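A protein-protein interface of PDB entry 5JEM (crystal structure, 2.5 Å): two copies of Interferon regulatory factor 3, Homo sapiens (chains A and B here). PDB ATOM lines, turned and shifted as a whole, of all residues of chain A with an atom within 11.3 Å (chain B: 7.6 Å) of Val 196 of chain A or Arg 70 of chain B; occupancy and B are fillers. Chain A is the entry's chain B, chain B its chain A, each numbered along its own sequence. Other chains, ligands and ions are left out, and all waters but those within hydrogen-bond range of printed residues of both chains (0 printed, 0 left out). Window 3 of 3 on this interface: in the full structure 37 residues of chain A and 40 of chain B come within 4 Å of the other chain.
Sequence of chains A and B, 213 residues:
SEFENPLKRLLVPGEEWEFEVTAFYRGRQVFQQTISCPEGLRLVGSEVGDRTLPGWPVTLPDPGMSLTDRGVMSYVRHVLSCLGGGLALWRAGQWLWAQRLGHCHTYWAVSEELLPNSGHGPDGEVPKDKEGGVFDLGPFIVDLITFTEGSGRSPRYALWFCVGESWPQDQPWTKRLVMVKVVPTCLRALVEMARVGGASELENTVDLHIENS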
ATOM      1  N   LEU A 144      -4.063 -20.463   1.431  1.00  0.00           N
ATOM      2  CA  LEU A 144      -4.375 -21.327   0.301  1.00  0.00           C
ATOM      3  C   LEU A 144      -5.318 -20.615  -0.665  1.00  0.00           C
ATOM      4  O   LEU A 144      -5.163 -20.706  -1.884  1.00  0.00           O
ATOM      5  CB  LEU A 144      -4.996 -22.638   0.786  1.00  0.00           C
ATOM      6  CG  LEU A 144      -5.423 -23.640  -0.289  1.00  0.00           C
ATOM      7  CD1 LEU A 144      -4.246 -23.981  -1.187  1.00  0.00           C
ATOM      8  CD2 LEU A 144      -6.005 -24.897   0.345  1.00  0.00           C
ATOM      9  N   PHE A 147      -3.522 -18.006  -2.446  1.00  0.00           N
ATOM     10  CA  PHE A 147      -2.651 -18.710  -3.378  1.00  0.00           C
ATOM     11  C   PHE A 147      -3.438 -19.052  -4.637  1.00  0.00           C
ATOM     12  O   PHE A 147      -2.956 -18.879  -5.759  1.00  0.00           O
ATOM     13  CB  PHE A 147      -2.076 -19.973  -2.736  1.00  0.00           C
ATOM     14  CG  PHE A 147      -1.169 -20.754  -3.640  1.00  0.00           C
ATOM     15  CD1 PHE A 147      -0.094 -20.142  -4.264  1.00  0.00           C
ATOM     16  CD2 PHE A 147      -1.383 -22.107  -3.858  1.00  0.00           C
ATOM     17  CE1 PHE A 147       0.747 -20.859  -5.098  1.00  0.00           C
ATOM     18  CE2 PHE A 147      -0.544 -22.832  -4.689  1.00  0.00           C
ATOM     19  CZ  PHE A 147       0.523 -22.204  -5.312  1.00  0.00           C
ATOM     20  N   THR A 148      -4.661 -19.531  -4.433  1.00  0.00           N
ATOM     21  CA  THR A 148      -5.590 -19.805  -5.524  1.00  0.00           C
ATOM     22  C   THR A 148      -5.857 -18.537  -6.343  1.00  0.00           C
ATOM     23  O   THR A 148      -6.027 -18.596  -7.562  1.00  0.00           O
ATOM     24  CB  THR A 148      -6.924 -20.393  -4.977  1.00  0.00           C
ATOM     25  OG1 THR A 148      -6.939 -21.813  -5.172  1.00  0.00           O
ATOM     26  CG2 THR A 148      -8.140 -19.776  -5.659  1.00  0.00           C
ATOM     27  N   SER A 154       2.734 -20.179  -1.859  1.00  0.00           N
ATOM     28  CA  SER A 154       2.103 -21.420  -1.436  1.00  0.00           C
ATOM     29  C   SER A 154       2.201 -21.604   0.078  1.00  0.00           C
ATOM     30  O   SER A 154       3.262 -21.393   0.666  1.00  0.00           O
ATOM     31  CB  SER A 154       2.740 -22.607  -2.157  1.00  0.00           C
ATOM     32  OG  SER A 154       2.093 -23.819  -1.821  1.00  0.00           O
ATOM     33  N   LEU A 187      -3.330 -31.917   3.624  1.00  0.00           N
ATOM     34  CA  LEU A 187      -2.957 -30.537   3.342  1.00  0.00           C
ATOM     35  C   LEU A 187      -2.096 -30.469   2.082  1.00  0.00           C
ATOM     36  O   LEU A 187      -2.206 -29.536   1.288  1.00  0.00           O
ATOM     37  CB  LEU A 187      -2.218 -29.921   4.530  1.00  0.00           C
ATOM     38  CG  LEU A 187      -3.014 -29.874   5.836  1.00  0.00           C
ATOM     39  CD1 LEU A 187      -2.253 -29.110   6.906  1.00  0.00           C
ATOM     40  CD2 LEU A 187      -4.392 -29.267   5.609  1.00  0.00           C
ATOM     41  N   ARG A 188      -1.239 -31.467   1.909  1.00  0.00           N
ATOM     42  CA  ARG A 188      -0.451 -31.588   0.691  1.00  0.00           C
ATOM     43  C   ARG A 188      -1.370 -31.705  -0.520  1.00  0.00           C
ATOM     44  O   ARG A 188      -1.114 -31.113  -1.570  1.00  0.00           O
ATOM     45  CB  ARG A 188       0.482 -32.797   0.771  1.00  0.00           C
ATOM     46  CG  ARG A 188       1.135 -33.169  -0.550  1.00  0.00           C
ATOM     47  CD  ARG A 188       1.778 -34.541  -0.464  1.00  0.00           C
ATOM     48  NE  ARG A 188       3.030 -34.518   0.285  1.00  0.00           N
ATOM     49  CZ  ARG A 188       3.609 -35.599   0.800  1.00  0.00           C
ATOM     50  NH1 ARG A 188       3.039 -36.788   0.662  1.00  0.00           N
ATOM     51  NH2 ARG A 188       4.754 -35.491   1.462  1.00  0.00           N
ATOM     52  N   ALA A 189      -2.447 -32.466  -0.358  1.00  0.00           N
ATOM     53  CA  ALA A 189      -3.394 -32.702  -1.437  1.00  0.00           C
ATOM     54  C   ALA A 189      -4.157 -31.429  -1.780  1.00  0.00           C
ATOM     55  O   ALA A 189      -4.454 -31.172  -2.948  1.00  0.00           O
ATOM     56  CB  ALA A 189      -4.356 -33.817  -1.063  1.00  0.00           C
ATOM     57  N   LEU A 190      -4.466 -30.636  -0.757  1.00  0.00           N
ATOM     58  CA  LEU A 190      -5.183 -29.377  -0.943  1.00  0.00           C
ATOM     59  C   LEU A 190      -4.374 -28.392  -1.788  1.00  0.00           C
ATOM     60  O   LEU A 190      -4.901 -27.777  -2.713  1.00  0.00           O
ATOM     61  CB  LEU A 190      -5.525 -28.749   0.410  1.00  0.00           C
ATOM     62  CG  LEU A 190      -6.984 -28.754   0.885  1.00  0.00           C
ATOM     63  CD1 LEU A 190      -7.913 -29.425  -0.121  1.00  0.00           C
ATOM     64  CD2 LEU A 190      -7.111 -29.405   2.258  1.00  0.00           C
ATOM     65  N   VAL A 191      -3.092 -28.250  -1.469  1.00  0.00           N
ATOM     66  CA  VAL A 191      -2.226 -27.346  -2.211  1.00  0.00           C
ATOM     67  C   VAL A 191      -2.044 -27.849  -3.641  1.00  0.00           C
ATOM     68  O   VAL A 191      -1.984 -27.059  -4.585  1.00  0.00           O
ATOM     69  CB  VAL A 191      -0.852 -27.192  -1.534  1.00  0.00           C
ATOM     70  CG1 VAL A 191      -0.019 -26.167  -2.266  1.00  0.00           C
ATOM     71  CG2 VAL A 191      -1.020 -26.783  -0.086  1.00  0.00           C
ATOM     72  N   GLU A 192      -1.968 -29.168  -3.799  1.00  0.00           N
ATOM     73  CA  GLU A 192      -1.883 -29.761  -5.129  1.00  0.00           C
ATOM     74  C   GLU A 192      -3.134 -29.430  -5.942  1.00  0.00           C
ATOM     75  O   GLU A 192      -3.050 -29.168  -7.141  1.00  0.00           O
ATOM     76  CB  GLU A 192      -1.691 -31.277  -5.045  1.00  0.00           C
ATOM     77  CG  GLU A 192      -1.747 -31.967  -6.402  1.00  0.00           C
ATOM     78  CD  GLU A 192      -1.325 -33.422  -6.354  1.00  0.00           C
ATOM     79  OE1 GLU A 192      -0.352 -33.743  -5.638  1.00  0.00           O
ATOM     80  OE2 GLU A 192      -1.970 -34.245  -7.036  1.00  0.00           O
ATOM     81  N   MET A 193      -4.289 -29.437  -5.280  1.00  0.00           N
ATOM     82  CA  MET A 193      -5.543 -29.056  -5.923  1.00  0.00           C
ATOM     83  C   MET A 193      -5.461 -27.641  -6.479  1.00  0.00           C
ATOM     84  O   MET A 193      -6.002 -27.350  -7.547  1.00  0.00           O
ATOM     85  CB  MET A 193      -6.712 -29.154  -4.941  1.00  0.00           C
ATOM     86  CG  MET A 193      -7.311 -30.541  -4.795  1.00  0.00           C
ATOM     87  SD  MET A 193      -8.668 -30.553  -3.598  1.00  0.00           S
ATOM     88  CE  MET A 193      -9.635 -29.166  -4.172  1.00  0.00           C
ATOM     89  N   ALA A 194      -4.785 -26.765  -5.743  1.00  0.00           N
ATOM     90  CA  ALA A 194      -4.612 -25.386  -6.173  1.00  0.00           C
ATOM     91  C   ALA A 194      -3.663 -25.316  -7.365  1.00  0.00           C
ATOM     92  O   ALA A 194      -3.875 -24.535  -8.290  1.00  0.00           O
ATOM     93  CB  ALA A 194      -4.102 -24.532  -5.027  1.00  0.00           C
ATOM     94  N   ARG A 195      -2.619 -26.141  -7.343  1.00  0.00           N
ATOM     95  CA  ARG A 195      -1.671 -26.182  -8.450  1.00  0.00           C
ATOM     96  C   ARG A 195      -2.351 -26.676  -9.722  1.00  0.00           C
ATOM     97  O   ARG A 195      -2.183 -26.090 -10.792  1.00  0.00           O
ATOM     98  CB  ARG A 195      -0.467 -27.068  -8.110  1.00  0.00           C
ATOM     99  CG  ARG A 195       0.543 -26.402  -7.192  1.00  0.00           C
ATOM    100  CD  ARG A 195       1.799 -27.242  -7.012  1.00  0.00           C
ATOM    101  NE  ARG A 195       1.994 -27.625  -5.618  1.00  0.00           N
ATOM    102  CZ  ARG A 195       1.803 -28.854  -5.149  1.00  0.00           C
ATOM    103  NH1 ARG A 195       1.427 -29.827  -5.969  1.00  0.00           N
ATOM    104  NH2 ARG A 195       1.996 -29.114  -3.862  1.00  0.00           N
ATOM    105  N   VAL A 196      -3.124 -27.748  -9.595  1.00  0.00           N
ATOM    106  CA  VAL A 196      -3.869 -28.297 -10.720  1.00  0.00           C
ATOM    107  C   VAL A 196      -4.890 -27.273 -11.211  1.00  0.00           C
ATOM    108  O   VAL A 196      -5.204 -27.209 -12.399  1.00  0.00           O
ATOM    109  CB  VAL A 196      -4.570 -29.621 -10.336  1.00  0.00           C
ATOM    110  CG1 VAL A 196      -5.443 -30.131 -11.472  1.00  0.00           C
ATOM    111  CG2 VAL A 196      -3.539 -30.671  -9.944  1.00  0.00           C
ATOM    112  N   GLY A 197      -5.382 -26.453 -10.288  1.00  0.00           N
ATOM    113  CA  GLY A 197      -6.315 -25.395 -10.627  1.00  0.00           C
ATOM    114  C   GLY A 197      -5.665 -24.257 -11.392  1.00  0.00           C
ATOM    115  O   GLY A 197      -6.352 -23.436 -12.000  1.00  0.00           O
ATOM    116  N   GLY A 198      -4.337 -24.200 -11.357  1.00  0.00           N
ATOM    117  CA  GLY A 198      -3.605 -23.207 -12.119  1.00  0.00           C
ATOM    118  C   GLY A 198      -2.744 -22.274 -11.289  1.00  0.00           C
ATOM    119  O   GLY A 198      -2.173 -21.321 -11.817  1.00  0.00           O
ATOM    120  N   ALA A 199      -2.651 -22.540  -9.991  1.00  0.00           N
ATOM    121  CA  ALA A 199      -1.804 -21.735  -9.120  1.00  0.00           C
ATOM    122  C   ALA A 199      -0.345 -22.129  -9.299  1.00  0.00           C
ATOM    123  O   ALA A 199      -0.026 -23.310  -9.447  1.00  0.00           O
ATOM    124  CB  ALA A 199      -2.226 -21.887  -7.668  1.00  0.00           C
ATOM    125  N   SER A 200       0.540 -21.138  -9.292  1.00  0.00           N
ATOM    126  CA  SER A 200       1.966 -21.398  -9.443  1.00  0.00           C
ATOM    127  C   SER A 200       2.773 -20.703  -8.352  1.00  0.00           C
ATOM    128  O   SER A 200       2.391 -19.634  -7.875  1.00  0.00           O
ATOM    129  CB  SER A 200       2.453 -20.946 -10.823  1.00  0.00           C
ATOM    130  OG  SER A 200       3.809 -21.311 -11.027  1.00  0.00           O
ATOM    131  N   GLU A 201       3.890 -21.315  -7.967  1.00  0.00           N
ATOM    132  CA  GLU A 201       4.766 -20.750  -6.948  1.00  0.00           C
ATOM    133  C   GLU A 201       5.952 -20.034  -7.584  1.00  0.00           C
ATOM    134  O   GLU A 201       6.789 -19.459  -6.886  1.00  0.00           O
ATOM    135  CB  GLU A 201       5.270 -21.841  -6.002  1.00  0.00           C
ATOM    136  CG  GLU A 201       4.187 -22.765  -5.474  1.00  0.00           C
ATOM    137  CD  GLU A 201       4.744 -23.869  -4.596  1.00  0.00           C
ATOM    138  OE1 GLU A 201       4.004 -24.836  -4.312  1.00  0.00           O
ATOM    139  OE2 GLU A 201       5.917 -23.763  -4.185  1.00  0.00           O
ATOM    140  N   LEU A 202       6.014 -20.074  -8.911  1.00  0.00           N
ATOM    141  CA  LEU A 202       7.145 -19.526  -9.649  1.00  0.00           C
ATOM    142  C   LEU A 202       7.295 -18.024  -9.434  1.00  0.00           C
ATOM    143  O   LEU A 202       6.372 -17.255  -9.695  1.00  0.00           O
ATOM    144  CB  LEU A 202       7.003 -19.826 -11.142  1.00  0.00           C
ATOM    145  CG  LEU A 202       8.223 -19.494 -12.002  1.00  0.00           C
ATOM    146  CD1 LEU A 202       9.399 -20.393 -11.644  1.00  0.00           C
ATOM    147  CD2 LEU A 202       7.888 -19.608 -13.475  1.00  0.00           C
ATOM    148  N   GLU A 203       8.467 -17.619  -8.955  1.00  0.00           N
ATOM    149  CA  GLU A 203       8.759 -16.215  -8.702  1.00  0.00           C
ATOM    150  C   GLU A 203       8.880 -15.452 -10.015  1.00  0.00           C
ATOM    151  O   GLU A 203       9.357 -15.994 -11.008  1.00  0.00           O
ATOM    152  CB  GLU A 203      10.049 -16.064  -7.890  1.00  0.00           C
ATOM    153  CG  GLU A 203      10.073 -16.845  -6.585  1.00  0.00           C
ATOM    154  CD  GLU A 203      10.449 -18.302  -6.773  1.00  0.00           C
ATOM    155  OE1 GLU A 203      11.129 -18.623  -7.771  1.00  0.00           O
ATOM    156  OE2 GLU A 203      10.060 -19.132  -5.925  1.00  0.00           O
ATOM    157  N   VAL A 206      12.519 -14.749 -11.870  1.00  0.00           N
ATOM    158  CA  VAL A 206      13.267 -15.782 -12.580  1.00  0.00           C
ATOM    159  C   VAL A 206      13.962 -15.207 -13.807  1.00  0.00           C
ATOM    160  O   VAL A 206      13.317 -14.691 -14.720  1.00  0.00           O
ATOM    161  CB  VAL A 206      12.362 -16.950 -13.011  1.00  0.00           C
ATOM    162  CG1 VAL A 206      13.104 -17.866 -13.971  1.00  0.00           C
ATOM    163  CG2 VAL A 206      11.889 -17.726 -11.797  1.00  0.00           C
ATOM    164  N   LEU B  67       5.363 -33.174 -11.948  1.00  0.00           N
ATOM    165  CA  LEU B  67       4.936 -31.915 -11.346  1.00  0.00           C
ATOM    166  C   LEU B  67       3.474 -31.573 -11.636  1.00  0.00           C
ATOM    167  O   LEU B  67       2.858 -32.147 -12.534  1.00  0.00           O
ATOM    168  CB  LEU B  67       5.833 -30.774 -11.830  1.00  0.00           C
ATOM    169  CG  LEU B  67       7.344 -31.016 -11.782  1.00  0.00           C
ATOM    170  CD1 LEU B  67       8.091 -29.762 -12.201  1.00  0.00           C
ATOM    171  CD2 LEU B  67       7.790 -31.473 -10.401  1.00  0.00           C
ATOM    172  N   THR B  68       2.927 -30.635 -10.866  1.00  0.00           N
ATOM    173  CA  THR B  68       1.578 -30.131 -11.103  1.00  0.00           C
ATOM    174  C   THR B  68       1.588 -28.618 -11.288  1.00  0.00           C
ATOM    175  O   THR B  68       0.645 -28.047 -11.831  1.00  0.00           O
ATOM    176  CB  THR B  68       0.611 -30.492  -9.955  1.00  0.00           C
ATOM    177  OG1 THR B  68       1.204 -30.158  -8.693  1.00  0.00           O
ATOM    178  CG2 THR B  68       0.279 -31.974  -9.980  1.00  0.00           C
ATOM    179  N   ASP B  69       2.657 -27.972 -10.832  1.00  0.00           N
ATOM    180  CA  ASP B  69       2.810 -26.534 -11.020  1.00  0.00           C
ATOM    181  C   ASP B  69       3.009 -26.219 -12.501  1.00  0.00           C
ATOM    182  O   ASP B  69       4.027 -26.578 -13.089  1.00  0.00           O
ATOM    183  CB  ASP B  69       3.983 -26.003 -10.189  1.00  0.00           C
ATOM    184  CG  ASP B  69       4.020 -24.484 -10.125  1.00  0.00           C
ATOM    185  OD1 ASP B  69       3.892 -23.826 -11.179  1.00  0.00           O
ATOM    186  OD2 ASP B  69       4.175 -23.945  -9.012  1.00  0.00           O
ATOM    187  N   ARG B  70       2.031 -25.545 -13.096  1.00  0.00           N
ATOM    188  CA  ARG B  70       2.057 -25.246 -14.524  1.00  0.00           C
ATOM    189  C   ARG B  70       3.155 -24.254 -14.890  1.00  0.00           C
ATOM    190  O   ARG B  70       3.790 -24.380 -15.937  1.00  0.00           O
ATOM    191  CB  ARG B  70       0.702 -24.704 -14.980  1.00  0.00           C
ATOM    192  CG  ARG B  70      -0.450 -25.677 -14.814  1.00  0.00           C
ATOM    193  CD  ARG B  70      -1.738 -25.080 -15.352  1.00  0.00           C
ATOM    194  NE  ARG B  70      -2.887 -25.946 -15.113  1.00  0.00           N
ATOM    195  CZ  ARG B  70      -4.134 -25.640 -15.456  1.00  0.00           C
ATOM    196  NH1 ARG B  70      -4.395 -24.485 -16.055  1.00  0.00           N
ATOM    197  NH2 ARG B  70      -5.121 -26.488 -15.201  1.00  0.00           N
ATOM    198  N   GLY B  71       3.366 -23.265 -14.028  1.00  0.00           N
ATOM    199  CA  GLY B  71       4.385 -22.258 -14.256  1.00  0.00           C
ATOM    200  C   GLY B  71       5.777 -22.858 -14.253  1.00  0.00           C
ATOM    201  O   GLY B  71       6.606 -22.542 -15.107  1.00  0.00           O
ATOM    202  N   VAL B  72       6.033 -23.729 -13.283  1.00  0.00           N
ATOM    203  CA  VAL B  72       7.305 -24.432 -13.209  1.00  0.00           C
ATOM    204  C   VAL B  72       7.454 -25.366 -14.405  1.00  0.00           C
ATOM    205  O   VAL B  72       8.524 -25.447 -15.010  1.00  0.00           O
ATOM    206  CB  VAL B  72       7.434 -25.236 -11.901  1.00  0.00           C
ATOM    207  CG1 VAL B  72       8.636 -26.157 -11.955  1.00  0.00           C
ATOM    208  CG2 VAL B  72       7.528 -24.296 -10.707  1.00  0.00           C
ATOM    209  N   MET B  73       6.368 -26.052 -14.749  1.00  0.00           N
ATOM    210  CA  MET B  73       6.371 -26.991 -15.866  1.00  0.00           C
ATOM    211  C   MET B  73       6.762 -26.306 -17.170  1.00  0.00           C
ATOM    212  O   MET B  73       7.530 -26.854 -17.960  1.00  0.00           O
ATOM    213  CB  MET B  73       5.003 -27.656 -16.014  1.00  0.00           C
ATOM    214  CG  MET B  73       5.024 -29.157 -15.763  1.00  0.00           C
ATOM    215  SD  MET B  73       3.390 -29.919 -15.837  1.00  0.00           S
ATOM    216  CE  MET B  73       2.527 -28.952 -14.612  1.00  0.00           C
ATOM    217  N   SER B  74       6.237 -25.105 -17.383  1.00  0.00           N
ATOM    218  CA  SER B  74       6.543 -24.334 -18.582  1.00  0.00           C
ATOM    219  C   SER B  74       8.027 -23.991 -18.673  1.00  0.00           C
ATOM    220  O   SER B  74       8.671 -24.245 -19.693  1.00  0.00           O
ATOM    221  CB  SER B  74       5.714 -23.050 -18.615  1.00  0.00           C
ATOM    222  OG  SER B  74       4.329 -23.341 -18.588  1.00  0.00           O
ATOM    223  N   TYR B  75       8.566 -23.419 -17.602  1.00  0.00           N
ATOM    224  CA  TYR B  75       9.951 -22.966 -17.601  1.00  0.00           C
ATOM    225  C   TYR B  75      10.951 -24.116 -17.653  1.00  0.00           C
ATOM    226  O   TYR B  75      12.001 -23.995 -18.277  1.00  0.00           O
ATOM    227  CB  TYR B  75      10.214 -22.091 -16.379  1.00  0.00           C
ATOM    228  CG  TYR B  75       9.841 -20.651 -16.617  1.00  0.00           C
ATOM    229  CD1 TYR B  75      10.815 -19.665 -16.695  1.00  0.00           C
ATOM    230  CD2 TYR B  75       8.514 -20.281 -16.804  1.00  0.00           C
ATOM    231  CE1 TYR B  75      10.476 -18.346 -16.929  1.00  0.00           C
ATOM    232  CE2 TYR B  75       8.165 -18.967 -17.038  1.00  0.00           C
ATOM    233  CZ  TYR B  75       9.148 -18.004 -17.100  1.00  0.00           C
ATOM    234  OH  TYR B  75       8.804 -16.693 -17.333  1.00  0.00           O
ATOM    235  N   VAL B  76      10.628 -25.229 -17.009  1.00  0.00           N
ATOM    236  CA  VAL B  76      11.493 -26.400 -17.074  1.00  0.00           C
ATOM    237  C   VAL B  76      11.530 -26.924 -18.510  1.00  0.00           C
ATOM    238  O   VAL B  76      12.599 -27.216 -19.044  1.00  0.00           O
ATOM    239  CB  VAL B  76      11.028 -27.515 -16.107  1.00  0.00           C
ATOM    240  CG1 VAL B  76      11.780 -28.812 -16.371  1.00  0.00           C
ATOM    241  CG2 VAL B  76      11.209 -27.078 -14.659  1.00  0.00           C
ATOM    242  N   ARG B  77      10.359 -27.023 -19.134  1.00  0.00           N
ATOM    243  CA  ARG B  77      10.256 -27.496 -20.513  1.00  0.00           C
ATOM    244  C   ARG B  77      11.069 -26.637 -21.470  1.00  0.00           C
ATOM    245  O   ARG B  77      11.684 -27.147 -22.405  1.00  0.00           O
ATOM    246  CB  ARG B  77       8.796 -27.524 -20.969  1.00  0.00           C
ATOM    247  CG  ARG B  77       8.032 -28.761 -20.544  1.00  0.00           C
ATOM    248  CD  ARG B  77       6.625 -28.765 -21.109  1.00  0.00           C
ATOM    249  NE  ARG B  77       5.869 -29.931 -20.669  1.00  0.00           N
ATOM    250  CZ  ARG B  77       4.694 -29.870 -20.052  1.00  0.00           C
ATOM    251  NH1 ARG B  77       4.130 -28.694 -19.808  1.00  0.00           N
ATOM    252  NH2 ARG B  77       4.076 -30.985 -19.685  1.00  0.00           N
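Printed residues of chain A that touch a printed residue of chain B: Arg 195, Val 196, Ser 200, Glu 201, Leu 202 and Val 206.
Hydrophobic or aromatic side chains of chain A within 4 Å of the printed part of chain B: Leu 202 and Val 206.
Arg 195 of chain A touches Asp 69 of chain B (CD to N, 3.98 Å).
OG of Ser 200 of chain A touches CA of Gly 71 of chain B (3.4 Å).
N of Val 72 of chain B touches OG of Ser 200 of chain A, at 3.99 Å.
CD2 of Leu 202 of chain A touches O of Gly 71 of chain B (3.6 Å).
CD2 of Tyr 75 of chain B touches CD2 of Leu 202 of chain A, at 3.5 Å.
Tyr 75 of chain B touches Val 206 of chain A.
Arg 70 of chain B touches just one residue of chain A: Val 196.
Printed residues of chain A within 4 Å of Thr 68 of chain B: Arg 195 (2.8 Å).
Gly 71 of chain B touches just these residues of chain A: Ser 200 (3.4 Å) and Leu 202 (3.6 Å).
No residue of chain A comes within 4 Å of Met 73 of chain B.
Printed residues of chain B within 4 Å of Arg 195 of chain A: Thr 68 (2.8 Å) and Asp 69 (3.98 Å).
Printed residues of chain B within 4 Å of Val 206 of chain A: Tyr 75 (3.99 Å).
Printed residues of chain B within 4 Å of Glu 201 of chain A: Asp 69 (2.8 Å).
Printed residues of chain B within 4 Å of Leu 202 of chain A: Gly 71 (3.6 Å) and Tyr 75 (3.5 Å).
Arg 188 of chain A touches none of the printed residues of chain B.
Ala 189 of chain A touches none of the printed residues of chain B.
The nearest printed residue of chain A that does not touch Tyr 75 of chain B is Glu 203 of chain A (6.4 Å).
The side-chain carboxylate of Asp 69 of chain B lies within hydrogen-bond range of the side-chain hydroxyl of Ser 200 of chain A, 2.5 Å away.
The backbone carbonyl oxygen (O) of Val 196 of chain A is in hydrogen-bond range of the guanidinium group (NH2) of Arg 70 of chain B.
The side-chain carboxylate of Asp 69 of chain B is in hydrogen-bond range of the backbone NH of Glu 201 of chain A.
The side-chain hydroxyl (OG1) of Thr 68 of chain B lies within hydrogen-bond range of the guanidinium group (NH1) of Arg 195 of chain A (2.8 Å).
The side-chain carboxylate of Glu 201 of chain A sits at hydrogen-bond distance from the side-chain hydroxyl of Ser 154 of chain A (3.3 Å).
The backbone NH (N) of Leu 202 of chain A lies within hydrogen-bond range of the side-chain hydroxyl (OG) of Ser 200 of chain A (3.3 Å).
The side-chain carboxylate (OD1) of Asp 69 of chain B lies within hydrogen-bond range of the backbone NH (N) of Val 72 of chain B.
NE of Arg 195 of chain A is in salt-bridge range of OE1 of Glu 201 of chain A, 3.7 Å away.
The backbone NH (N) of Gly 71 of chain B sits at hydrogen-bond distance from the side-chain carboxylate (OD1) of Asp 69 of chain B (3.0 Å).
The backbone carbonyl oxygen (O) of Arg 70 of chain B is in hydrogen-bond range of the side-chain hydroxyl (OG) of Ser 74 of chain B, at 2.9 Å.
No position is printed for both chains.
Of the 10 pairs that touch across the chains among the printed residues, none has its exchanged pair printed and touching as well.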
